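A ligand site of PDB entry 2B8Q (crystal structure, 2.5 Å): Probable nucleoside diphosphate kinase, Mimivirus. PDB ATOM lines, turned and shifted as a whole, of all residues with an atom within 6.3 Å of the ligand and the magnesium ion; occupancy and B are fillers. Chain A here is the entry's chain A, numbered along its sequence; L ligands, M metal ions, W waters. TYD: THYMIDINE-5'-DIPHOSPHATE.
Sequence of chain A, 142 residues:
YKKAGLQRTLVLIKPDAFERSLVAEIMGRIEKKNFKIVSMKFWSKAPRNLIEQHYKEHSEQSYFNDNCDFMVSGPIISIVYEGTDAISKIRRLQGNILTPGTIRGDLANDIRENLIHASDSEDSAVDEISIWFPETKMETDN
NZ of Lys 14 lies within hydrogen-bond range of O3' of the ligand. O3' of the ligand sits at hydrogen-bond distance from ND2 of Asn 114, at 2.9 Å. The guanidinium group (NH1) of Arg 104 is in salt-bridge range of an oxygen (O3B) of the ligand (2.5 Å). The guanidinium group of Arg 91 is in salt-bridge range of an oxygen (O2B) of the ligand. OD1 of Asn 67 sits close to O4' of the ligand (3.4 Å).
OD1 of Asn 114 is in hydrogen-bond range of NZ of Lys 14. NH1 of Arg 104 sits close to ND2 of Asn 114 (3.4 Å). O of Gln 94 lies within hydrogen-bond range of N of Arg 104 (3.1 Å). NZ of Lys 14 lies within hydrogen-bond range of OH of Tyr 55, 3.1 Å away. The side-chain hydroxyl (OH) of Tyr 63 is in hydrogen-bond range of a ring nitrogen (ND1) of His 58 (2.5 Å). The backbone carbonyl oxygen (O) of Ile 116 is in hydrogen-bond range of the guanidinium group (NH2) of Arg 104 (2.7 Å). The side-chain amide oxygen (OE1) of Gln 94 is in hydrogen-bond range of the backbone NH (N) of Ala 118, at 2.9 Å.
Water W1 lies within hydrogen-bond range of ND2 of Asn 67, O of Arg 112 and NZ of Lys 14.
The magnesium ion is bound by O1A of the ligand (2.5 Å). The magnesium ion has one donor atom within binding distance. Slightly farther from the magnesium ion lies O2B of the ligand (2.7 Å).
His 58 touches the magnesium ion. Arg 91 touches the magnesium ion. Of the 21 residues printed, 2 come within 4 Å of the magnesium ion. Along chain A the residues within 4 Å of the magnesium ion span positions 58 to 91.
Residues that only touch the ligand: Tyr 55 (3.8 Å), His 58 (3.5 Å), Tyr 63 (3.4 Å), Gln 94 (3.7 Å), Ile 111 (3.7 Å) and Arg 112 (3.1 Å). Hydrophobic or aromatic side chains within 4 Å of the ligand: Tyr 55, His 58 and Tyr 63. Within 4 Å of the ligand: Lys 14, Tyr 55, His 58, Tyr 63, Asn 67, Arg 91, Gln 94, Arg 104, Ile 111, Arg 112 and Asn 114. The nearest printed residue that does not touch the ligand is His 117 (4.8 Å).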
ATOM      1  N   LYS A  14      22.529 -26.824   6.269  1.00  0.00           N
ATOM      2  CA  LYS A  14      22.898 -26.490   7.638  1.00  0.00           C
ATOM      3  C   LYS A  14      24.265 -26.983   8.127  1.00  0.00           C
ATOM      4  O   LYS A  14      24.898 -27.827   7.501  1.00  0.00           O
ATOM      5  CB  LYS A  14      21.764 -26.948   8.561  1.00  0.00           C
ATOM      6  CG  LYS A  14      20.407 -26.383   8.138  1.00  0.00           C
ATOM      7  CD  LYS A  14      19.325 -26.749   9.125  1.00  0.00           C
ATOM      8  CE  LYS A  14      18.022 -25.996   8.848  1.00  0.00           C
ATOM      9  NZ  LYS A  14      16.961 -26.323   9.855  1.00  0.00           N
ATOM     10  N   TYR A  55      14.208 -17.076  10.631  1.00  0.00           N
ATOM     11  CA  TYR A  55      13.308 -17.758  11.539  1.00  0.00           C
ATOM     12  C   TYR A  55      12.479 -16.810  12.413  1.00  0.00           C
ATOM     13  O   TYR A  55      12.024 -17.206  13.481  1.00  0.00           O
ATOM     14  CB  TYR A  55      14.087 -18.700  12.454  1.00  0.00           C
ATOM     15  CG  TYR A  55      14.643 -19.910  11.744  1.00  0.00           C
ATOM     16  CD1 TYR A  55      16.015 -20.065  11.543  1.00  0.00           C
ATOM     17  CD2 TYR A  55      13.797 -20.931  11.289  1.00  0.00           C
ATOM     18  CE1 TYR A  55      16.536 -21.188  10.911  1.00  0.00           C
ATOM     19  CE2 TYR A  55      14.307 -22.062  10.653  1.00  0.00           C
ATOM     20  CZ  TYR A  55      15.680 -22.186  10.472  1.00  0.00           C
ATOM     21  OH  TYR A  55      16.184 -23.295   9.838  1.00  0.00           O
ATOM     22  N   GLU A  57       9.468 -15.880  12.325  1.00  0.00           N
ATOM     23  CA  GLU A  57       8.160 -16.429  12.663  1.00  0.00           C
ATOM     24  C   GLU A  57       8.225 -17.347  13.897  1.00  0.00           C
ATOM     25  O   GLU A  57       7.216 -17.606  14.543  1.00  0.00           O
ATOM     26  CB  GLU A  57       7.594 -17.216  11.476  1.00  0.00           C
ATOM     27  CG  GLU A  57       7.406 -16.398  10.196  1.00  0.00           C
ATOM     28  CD  GLU A  57       7.115 -17.269   8.959  1.00  0.00           C
ATOM     29  OE1 GLU A  57       7.998 -18.076   8.573  1.00  0.00           O
ATOM     30  OE2 GLU A  57       6.011 -17.146   8.376  1.00  0.00           O
ATOM     31  N   HIS A  58       9.424 -17.826  14.219  1.00  0.00           N
ATOM     32  CA  HIS A  58       9.645 -18.713  15.367  1.00  0.00           C
ATOM     33  C   HIS A  58      10.178 -17.985  16.608  1.00  0.00           C
ATOM     34  O   HIS A  58      10.490 -18.624  17.620  1.00  0.00           O
ATOM     35  CB  HIS A  58      10.643 -19.809  14.987  1.00  0.00           C
ATOM     36  CG  HIS A  58      10.224 -20.661  13.835  1.00  0.00           C
ATOM     37  ND1 HIS A  58       9.572 -21.871  14.002  1.00  0.00           N
ATOM     38  CD2 HIS A  58      10.347 -20.492  12.500  1.00  0.00           C
ATOM     39  CE1 HIS A  58       9.322 -22.390  12.821  1.00  0.00           C
ATOM     40  NE2 HIS A  58       9.782 -21.580  11.888  1.00  0.00           N
ATOM     41  N   TYR A  63      12.388 -23.212  21.573  1.00  0.00           N
ATOM     42  CA  TYR A  63      13.578 -23.675  20.852  1.00  0.00           C
ATOM     43  C   TYR A  63      14.264 -22.619  20.004  1.00  0.00           C
ATOM     44  O   TYR A  63      15.349 -22.864  19.486  1.00  0.00           O
ATOM     45  CB  TYR A  63      13.196 -24.863  19.947  1.00  0.00           C
ATOM     46  CG  TYR A  63      12.192 -24.517  18.861  1.00  0.00           C
ATOM     47  CD1 TYR A  63      12.572 -23.739  17.762  1.00  0.00           C
ATOM     48  CD2 TYR A  63      10.858 -24.920  18.960  1.00  0.00           C
ATOM     49  CE1 TYR A  63      11.645 -23.380  16.781  1.00  0.00           C
ATOM     50  CE2 TYR A  63       9.931 -24.561  17.979  1.00  0.00           C
ATOM     51  CZ  TYR A  63      10.326 -23.792  16.902  1.00  0.00           C
ATOM     52  OH  TYR A  63       9.408 -23.408  15.952  1.00  0.00           O
ATOM     53  N   PHE A  64      13.636 -21.451  19.888  1.00  0.00           N
ATOM     54  CA  PHE A  64      14.159 -20.366  19.065  1.00  0.00           C
ATOM     55  C   PHE A  64      15.611 -19.916  19.230  1.00  0.00           C
ATOM     56  O   PHE A  64      16.267 -19.619  18.228  1.00  0.00           O
ATOM     57  CB  PHE A  64      13.270 -19.139  19.161  1.00  0.00           C
ATOM     58  CG  PHE A  64      13.730 -17.991  18.307  1.00  0.00           C
ATOM     59  CD1 PHE A  64      14.497 -16.965  18.837  1.00  0.00           C
ATOM     60  CD2 PHE A  64      13.445 -17.968  16.941  1.00  0.00           C
ATOM     61  CE1 PHE A  64      14.963 -15.925  18.035  1.00  0.00           C
ATOM     62  CE2 PHE A  64      13.908 -16.933  16.130  1.00  0.00           C
ATOM     63  CZ  PHE A  64      14.677 -15.910  16.685  1.00  0.00           C
ATOM     64  N   ASP A  66      18.213 -21.710  20.872  1.00  0.00           N
ATOM     65  CA  ASP A  66      19.152 -22.813  20.683  1.00  0.00           C
ATOM     66  C   ASP A  66      19.298 -23.089  19.182  1.00  0.00           C
ATOM     67  O   ASP A  66      20.382 -23.389  18.715  1.00  0.00           O
ATOM     68  CB  ASP A  66      18.657 -24.086  21.376  1.00  0.00           C
ATOM     69  CG  ASP A  66      18.670 -23.960  22.879  1.00  0.00           C
ATOM     70  OD1 ASP A  66      19.703 -23.493  23.420  1.00  0.00           O
ATOM     71  OD2 ASP A  66      17.654 -24.338  23.527  1.00  0.00           O
ATOM     72  N   ASN A  67      18.202 -22.963  18.441  1.00  0.00           N
ATOM     73  CA  ASN A  67      18.239 -23.194  17.007  1.00  0.00           C
ATOM     74  C   ASN A  67      19.152 -22.167  16.335  1.00  0.00           C
ATOM     75  O   ASN A  67      19.840 -22.486  15.356  1.00  0.00           O
ATOM     76  CB  ASN A  67      16.836 -23.102  16.401  1.00  0.00           C
ATOM     77  CG  ASN A  67      16.822 -23.485  14.931  1.00  0.00           C
ATOM     78  OD1 ASN A  67      16.188 -22.826  14.103  1.00  0.00           O
ATOM     79  ND2 ASN A  67      17.535 -24.548  14.597  1.00  0.00           N
ATOM     80  N   ARG A  91      10.354 -29.169  -1.005  1.00  0.00           N
ATOM     81  CA  ARG A  91       9.875 -29.322   0.364  1.00  0.00           C
ATOM     82  C   ARG A  91       9.618 -30.794   0.653  1.00  0.00           C
ATOM     83  O   ARG A  91       9.950 -31.287   1.727  1.00  0.00           O
ATOM     84  CB  ARG A  91       8.598 -28.511   0.580  1.00  0.00           C
ATOM     85  CG  ARG A  91       8.732 -27.492   1.687  1.00  0.00           C
ATOM     86  CD  ARG A  91       8.313 -28.071   3.010  1.00  0.00           C
ATOM     87  NE  ARG A  91       9.007 -27.407   4.114  1.00  0.00           N
ATOM     88  CZ  ARG A  91       8.578 -27.408   5.365  1.00  0.00           C
ATOM     89  NH1 ARG A  91       7.444 -28.017   5.678  1.00  0.00           N
ATOM     90  NH2 ARG A  91       9.292 -26.798   6.299  1.00  0.00           N
ATOM     91  N   GLN A  94      12.808 -32.627   1.026  1.00  0.00           N
ATOM     92  CA  GLN A  94      13.353 -32.398   2.369  1.00  0.00           C
ATOM     93  C   GLN A  94      12.697 -33.363   3.348  1.00  0.00           C
ATOM     94  O   GLN A  94      13.372 -33.952   4.186  1.00  0.00           O
ATOM     95  CB  GLN A  94      13.058 -30.969   2.822  1.00  0.00           C
ATOM     96  CG  GLN A  94      13.342 -30.718   4.289  1.00  0.00           C
ATOM     97  CD  GLN A  94      12.715 -29.433   4.787  1.00  0.00           C
ATOM     98  OE1 GLN A  94      13.118 -28.341   4.420  1.00  0.00           O
ATOM     99  NE2 GLN A  94      11.715 -29.573   5.653  1.00  0.00           N
ATOM    100  N   GLY A  95      11.377 -33.501   3.226  1.00  0.00           N
ATOM    101  CA  GLY A  95      10.623 -34.400   4.092  1.00  0.00           C
ATOM    102  C   GLY A  95      10.924 -34.142   5.549  1.00  0.00           C
ATOM    103  O   GLY A  95      11.244 -33.013   5.940  1.00  0.00           O
ATOM    104  N   ASN A  96      10.804 -35.185   6.374  1.00  0.00           N
ATOM    105  CA  ASN A  96      11.066 -35.073   7.800  1.00  0.00           C
ATOM    106  C   ASN A  96      11.786 -36.325   8.289  1.00  0.00           C
ATOM    107  O   ASN A  96      11.930 -37.283   7.529  1.00  0.00           O
ATOM    108  CB  ASN A  96       9.754 -34.871   8.593  1.00  0.00           C
ATOM    109  CG  ASN A  96       8.663 -35.874   8.223  1.00  0.00           C
ATOM    110  OD1 ASN A  96       8.829 -37.085   8.360  1.00  0.00           O
ATOM    111  ND2 ASN A  96       7.535 -35.359   7.749  1.00  0.00           N
ATOM    112  N   ARG A 104      15.754 -35.728   5.030  1.00  0.00           N
ATOM    113  CA  ARG A 104      15.788 -35.851   6.483  1.00  0.00           C
ATOM    114  C   ARG A 104      15.435 -37.271   6.912  1.00  0.00           C
ATOM    115  O   ARG A 104      15.955 -37.767   7.892  1.00  0.00           O
ATOM    116  CB  ARG A 104      14.814 -34.870   7.136  1.00  0.00           C
ATOM    117  CG  ARG A 104      15.257 -33.431   7.077  1.00  0.00           C
ATOM    118  CD  ARG A 104      14.230 -32.554   7.743  1.00  0.00           C
ATOM    119  NE  ARG A 104      14.523 -31.138   7.634  1.00  0.00           N
ATOM    120  CZ  ARG A 104      13.782 -30.201   8.208  1.00  0.00           C
ATOM    121  NH1 ARG A 104      12.726 -30.560   8.945  1.00  0.00           N
ATOM    122  NH2 ARG A 104      14.072 -28.914   8.059  1.00  0.00           N
ATOM    123  N   ILE A 111      15.564 -33.102  16.161  1.00  0.00           N
ATOM    124  CA  ILE A 111      14.569 -32.047  15.981  1.00  0.00           C
ATOM    125  C   ILE A 111      15.186 -30.737  15.553  1.00  0.00           C
ATOM    126  O   ILE A 111      14.521 -29.897  14.953  1.00  0.00           O
ATOM    127  CB  ILE A 111      13.782 -31.784  17.286  1.00  0.00           C
ATOM    128  CG1 ILE A 111      14.749 -31.815  18.477  1.00  0.00           C
ATOM    129  CG2 ILE A 111      12.633 -32.780  17.419  1.00  0.00           C
ATOM    130  CD1 ILE A 111      14.086 -31.646  19.840  1.00  0.00           C
ATOM    131  N   ARG A 112      16.466 -30.563  15.862  1.00  0.00           N
ATOM    132  CA  ARG A 112      17.165 -29.318  15.541  1.00  0.00           C
ATOM    133  C   ARG A 112      18.223 -29.486  14.440  1.00  0.00           C
ATOM    134  O   ARG A 112      18.296 -28.670  13.522  1.00  0.00           O
ATOM    135  CB  ARG A 112      17.816 -28.775  16.817  1.00  0.00           C
ATOM    136  CG  ARG A 112      18.339 -27.339  16.728  1.00  0.00           C
ATOM    137  CD  ARG A 112      19.172 -26.986  17.957  1.00  0.00           C
ATOM    138  NE  ARG A 112      20.532 -27.539  17.877  1.00  0.00           N
ATOM    139  CZ  ARG A 112      21.372 -27.639  18.903  1.00  0.00           C
ATOM    140  NH1 ARG A 112      21.006 -27.225  20.113  1.00  0.00           N
ATOM    141  NH2 ARG A 112      22.597 -28.141  18.719  1.00  0.00           N
ATOM    142  N   GLU A 113      19.053 -30.517  14.552  1.00  0.00           N
ATOM    143  CA  GLU A 113      20.087 -30.759  13.556  1.00  0.00           C
ATOM    144  C   GLU A 113      19.509 -31.638  12.467  1.00  0.00           C
ATOM    145  O   GLU A 113      19.741 -32.853  12.439  1.00  0.00           O
ATOM    146  CB  GLU A 113      21.307 -31.414  14.217  1.00  0.00           C
ATOM    147  CG  GLU A 113      21.974 -30.501  15.231  1.00  0.00           C
ATOM    148  CD  GLU A 113      23.135 -31.141  15.967  1.00  0.00           C
ATOM    149  OE1 GLU A 113      22.912 -32.203  16.593  1.00  0.00           O
ATOM    150  OE2 GLU A 113      24.255 -30.593  15.938  1.00  0.00           O
ATOM    151  N   ASN A 114      18.752 -31.018  11.563  1.00  0.00           N
ATOM    152  CA  ASN A 114      18.100 -31.735  10.481  1.00  0.00           C
ATOM    153  C   ASN A 114      18.623 -31.453   9.078  1.00  0.00           C
ATOM    154  O   ASN A 114      17.884 -31.552   8.111  1.00  0.00           O
ATOM    155  CB  ASN A 114      16.592 -31.512  10.523  1.00  0.00           C
ATOM    156  CG  ASN A 114      16.231 -30.063  10.696  1.00  0.00           C
ATOM    157  OD1 ASN A 114      16.986 -29.171  10.305  1.00  0.00           O
ATOM    158  ND2 ASN A 114      15.052 -29.816  11.261  1.00  0.00           N
ATOM    159  N   ILE A 116      18.845 -29.605   6.562  1.00  0.00           N
ATOM    160  CA  ILE A 116      18.390 -28.713   5.512  1.00  0.00           C
ATOM    161  C   ILE A 116      17.101 -27.937   5.750  1.00  0.00           C
ATOM    162  O   ILE A 116      16.201 -28.391   6.451  1.00  0.00           O
ATOM    163  CB  ILE A 116      18.224 -29.542   4.205  1.00  0.00           C
ATOM    164  CG1 ILE A 116      17.655 -28.686   3.077  1.00  0.00           C
ATOM    165  CG2 ILE A 116      17.322 -30.733   4.471  1.00  0.00           C
ATOM    166  CD1 ILE A 116      17.410 -29.475   1.803  1.00  0.00           C
ATOM    167  N   HIS A 117      17.033 -26.761   5.144  1.00  0.00           N
ATOM    168  CA  HIS A 117      15.845 -25.920   5.193  1.00  0.00           C
ATOM    169  C   HIS A 117      15.378 -25.657   3.777  1.00  0.00           C
ATOM    170  O   HIS A 117      16.179 -25.421   2.868  1.00  0.00           O
ATOM    171  CB  HIS A 117      16.126 -24.570   5.842  1.00  0.00           C
ATOM    172  CG  HIS A 117      14.998 -23.611   5.644  1.00  0.00           C
ATOM    173  ND1 HIS A 117      13.908 -23.548   6.491  1.00  0.00           N
ATOM    174  CD2 HIS A 117      14.720 -22.759   4.630  1.00  0.00           C
ATOM    175  CE1 HIS A 117      13.009 -22.711   6.006  1.00  0.00           C
ATOM    176  NE2 HIS A 117      13.480 -22.222   4.873  1.00  0.00           N
ATOM    177  N   ALA A 118      14.056 -25.675   3.595  1.00  0.00           N
ATOM    178  CA  ALA A 118      13.448 -25.400   2.298  1.00  0.00           C
ATOM    179  C   ALA A 118      12.191 -24.579   2.513  1.00  0.00           C
ATOM    180  O   ALA A 118      11.385 -24.886   3.389  1.00  0.00           O
ATOM    181  CB  ALA A 118      13.113 -26.707   1.577  1.00  0.00           C
ATOM    182  N   ASP A 120       8.589 -23.218   2.615  1.00  0.00           N
ATOM    183  CA  ASP A 120       7.355 -23.992   2.623  1.00  0.00           C
ATOM    184  C   ASP A 120       6.173 -23.350   1.894  1.00  0.00           C
ATOM    185  O   ASP A 120       5.073 -23.888   1.922  1.00  0.00           O
ATOM    186  CB  ASP A 120       6.944 -24.348   4.055  1.00  0.00           C
ATOM    187  CG  ASP A 120       6.465 -23.154   4.850  1.00  0.00           C
ATOM    188  OD1 ASP A 120       6.437 -22.026   4.287  1.00  0.00           O
ATOM    189  OD2 ASP A 120       6.112 -23.345   6.036  1.00  0.00           O
HETATM  190  PA  TYD L   1       9.867 -26.319  11.863  1.00  0.00           P
HETATM  191  O1A TYD L   1       9.112 -25.367  11.018  1.00  0.00           O
HETATM  192  O2A TYD L   1       8.925 -27.008  12.969  1.00  0.00           O
HETATM  193  O3A TYD L   1      10.495 -27.553  11.032  1.00  0.00           O
HETATM  194  PB  TYD L   1      10.969 -27.454   9.490  1.00  0.00           P
HETATM  195  O1B TYD L   1      12.304 -26.829   9.659  1.00  0.00           O
HETATM  196  O2B TYD L   1       9.697 -26.625   8.951  1.00  0.00           O
HETATM  197  O3B TYD L   1      10.778 -29.036   9.229  1.00  0.00           O
HETATM  198  O5' TYD L   1      11.070 -25.645  12.685  1.00  0.00           O
HETATM  199  C5' TYD L   1      12.068 -24.893  11.999  1.00  0.00           C
HETATM  200  C4' TYD L   1      13.429 -25.116  12.663  1.00  0.00           C
HETATM  201  O4' TYD L   1      13.424 -24.731  14.056  1.00  0.00           O
HETATM  202  C3' TYD L   1      13.773 -26.605  12.693  1.00  0.00           C
HETATM  203  O3' TYD L   1      14.234 -27.005  11.404  1.00  0.00           O
HETATM  204  C2' TYD L   1      14.951 -26.505  13.656  1.00  0.00           C
HETATM  205  C1' TYD L   1      14.347 -25.602  14.737  1.00  0.00           C
HETATM  206  N1  TYD L   1      13.598 -26.398  15.739  1.00  0.00           N
HETATM  207  C2  TYD L   1      14.232 -26.785  16.929  1.00  0.00           C
HETATM  208  O2  TYD L   1      15.404 -26.471  17.150  1.00  0.00           O
HETATM  209  N3  TYD L   1      13.520 -27.519  17.885  1.00  0.00           N
HETATM  210  C4  TYD L   1      12.175 -27.866  17.653  1.00  0.00           C
HETATM  211  O4  TYD L   1      11.563 -28.498  18.509  1.00  0.00           O
HETATM  212  C5  TYD L   1      11.548 -27.483  16.474  1.00  0.00           C
HETATM  213  C5M TYD L   1      10.078 -27.841  16.224  1.00  0.00           C
HETATM  214  C6  TYD L   1      12.252 -26.753  15.522  1.00  0.00           C
HETATM  215 MG    MG M   1       9.538 -23.951   8.993  1.00  0.00          MG
HETATM  216  O   HOH W   1      18.005 -26.165  12.576  1.00  0.00           O
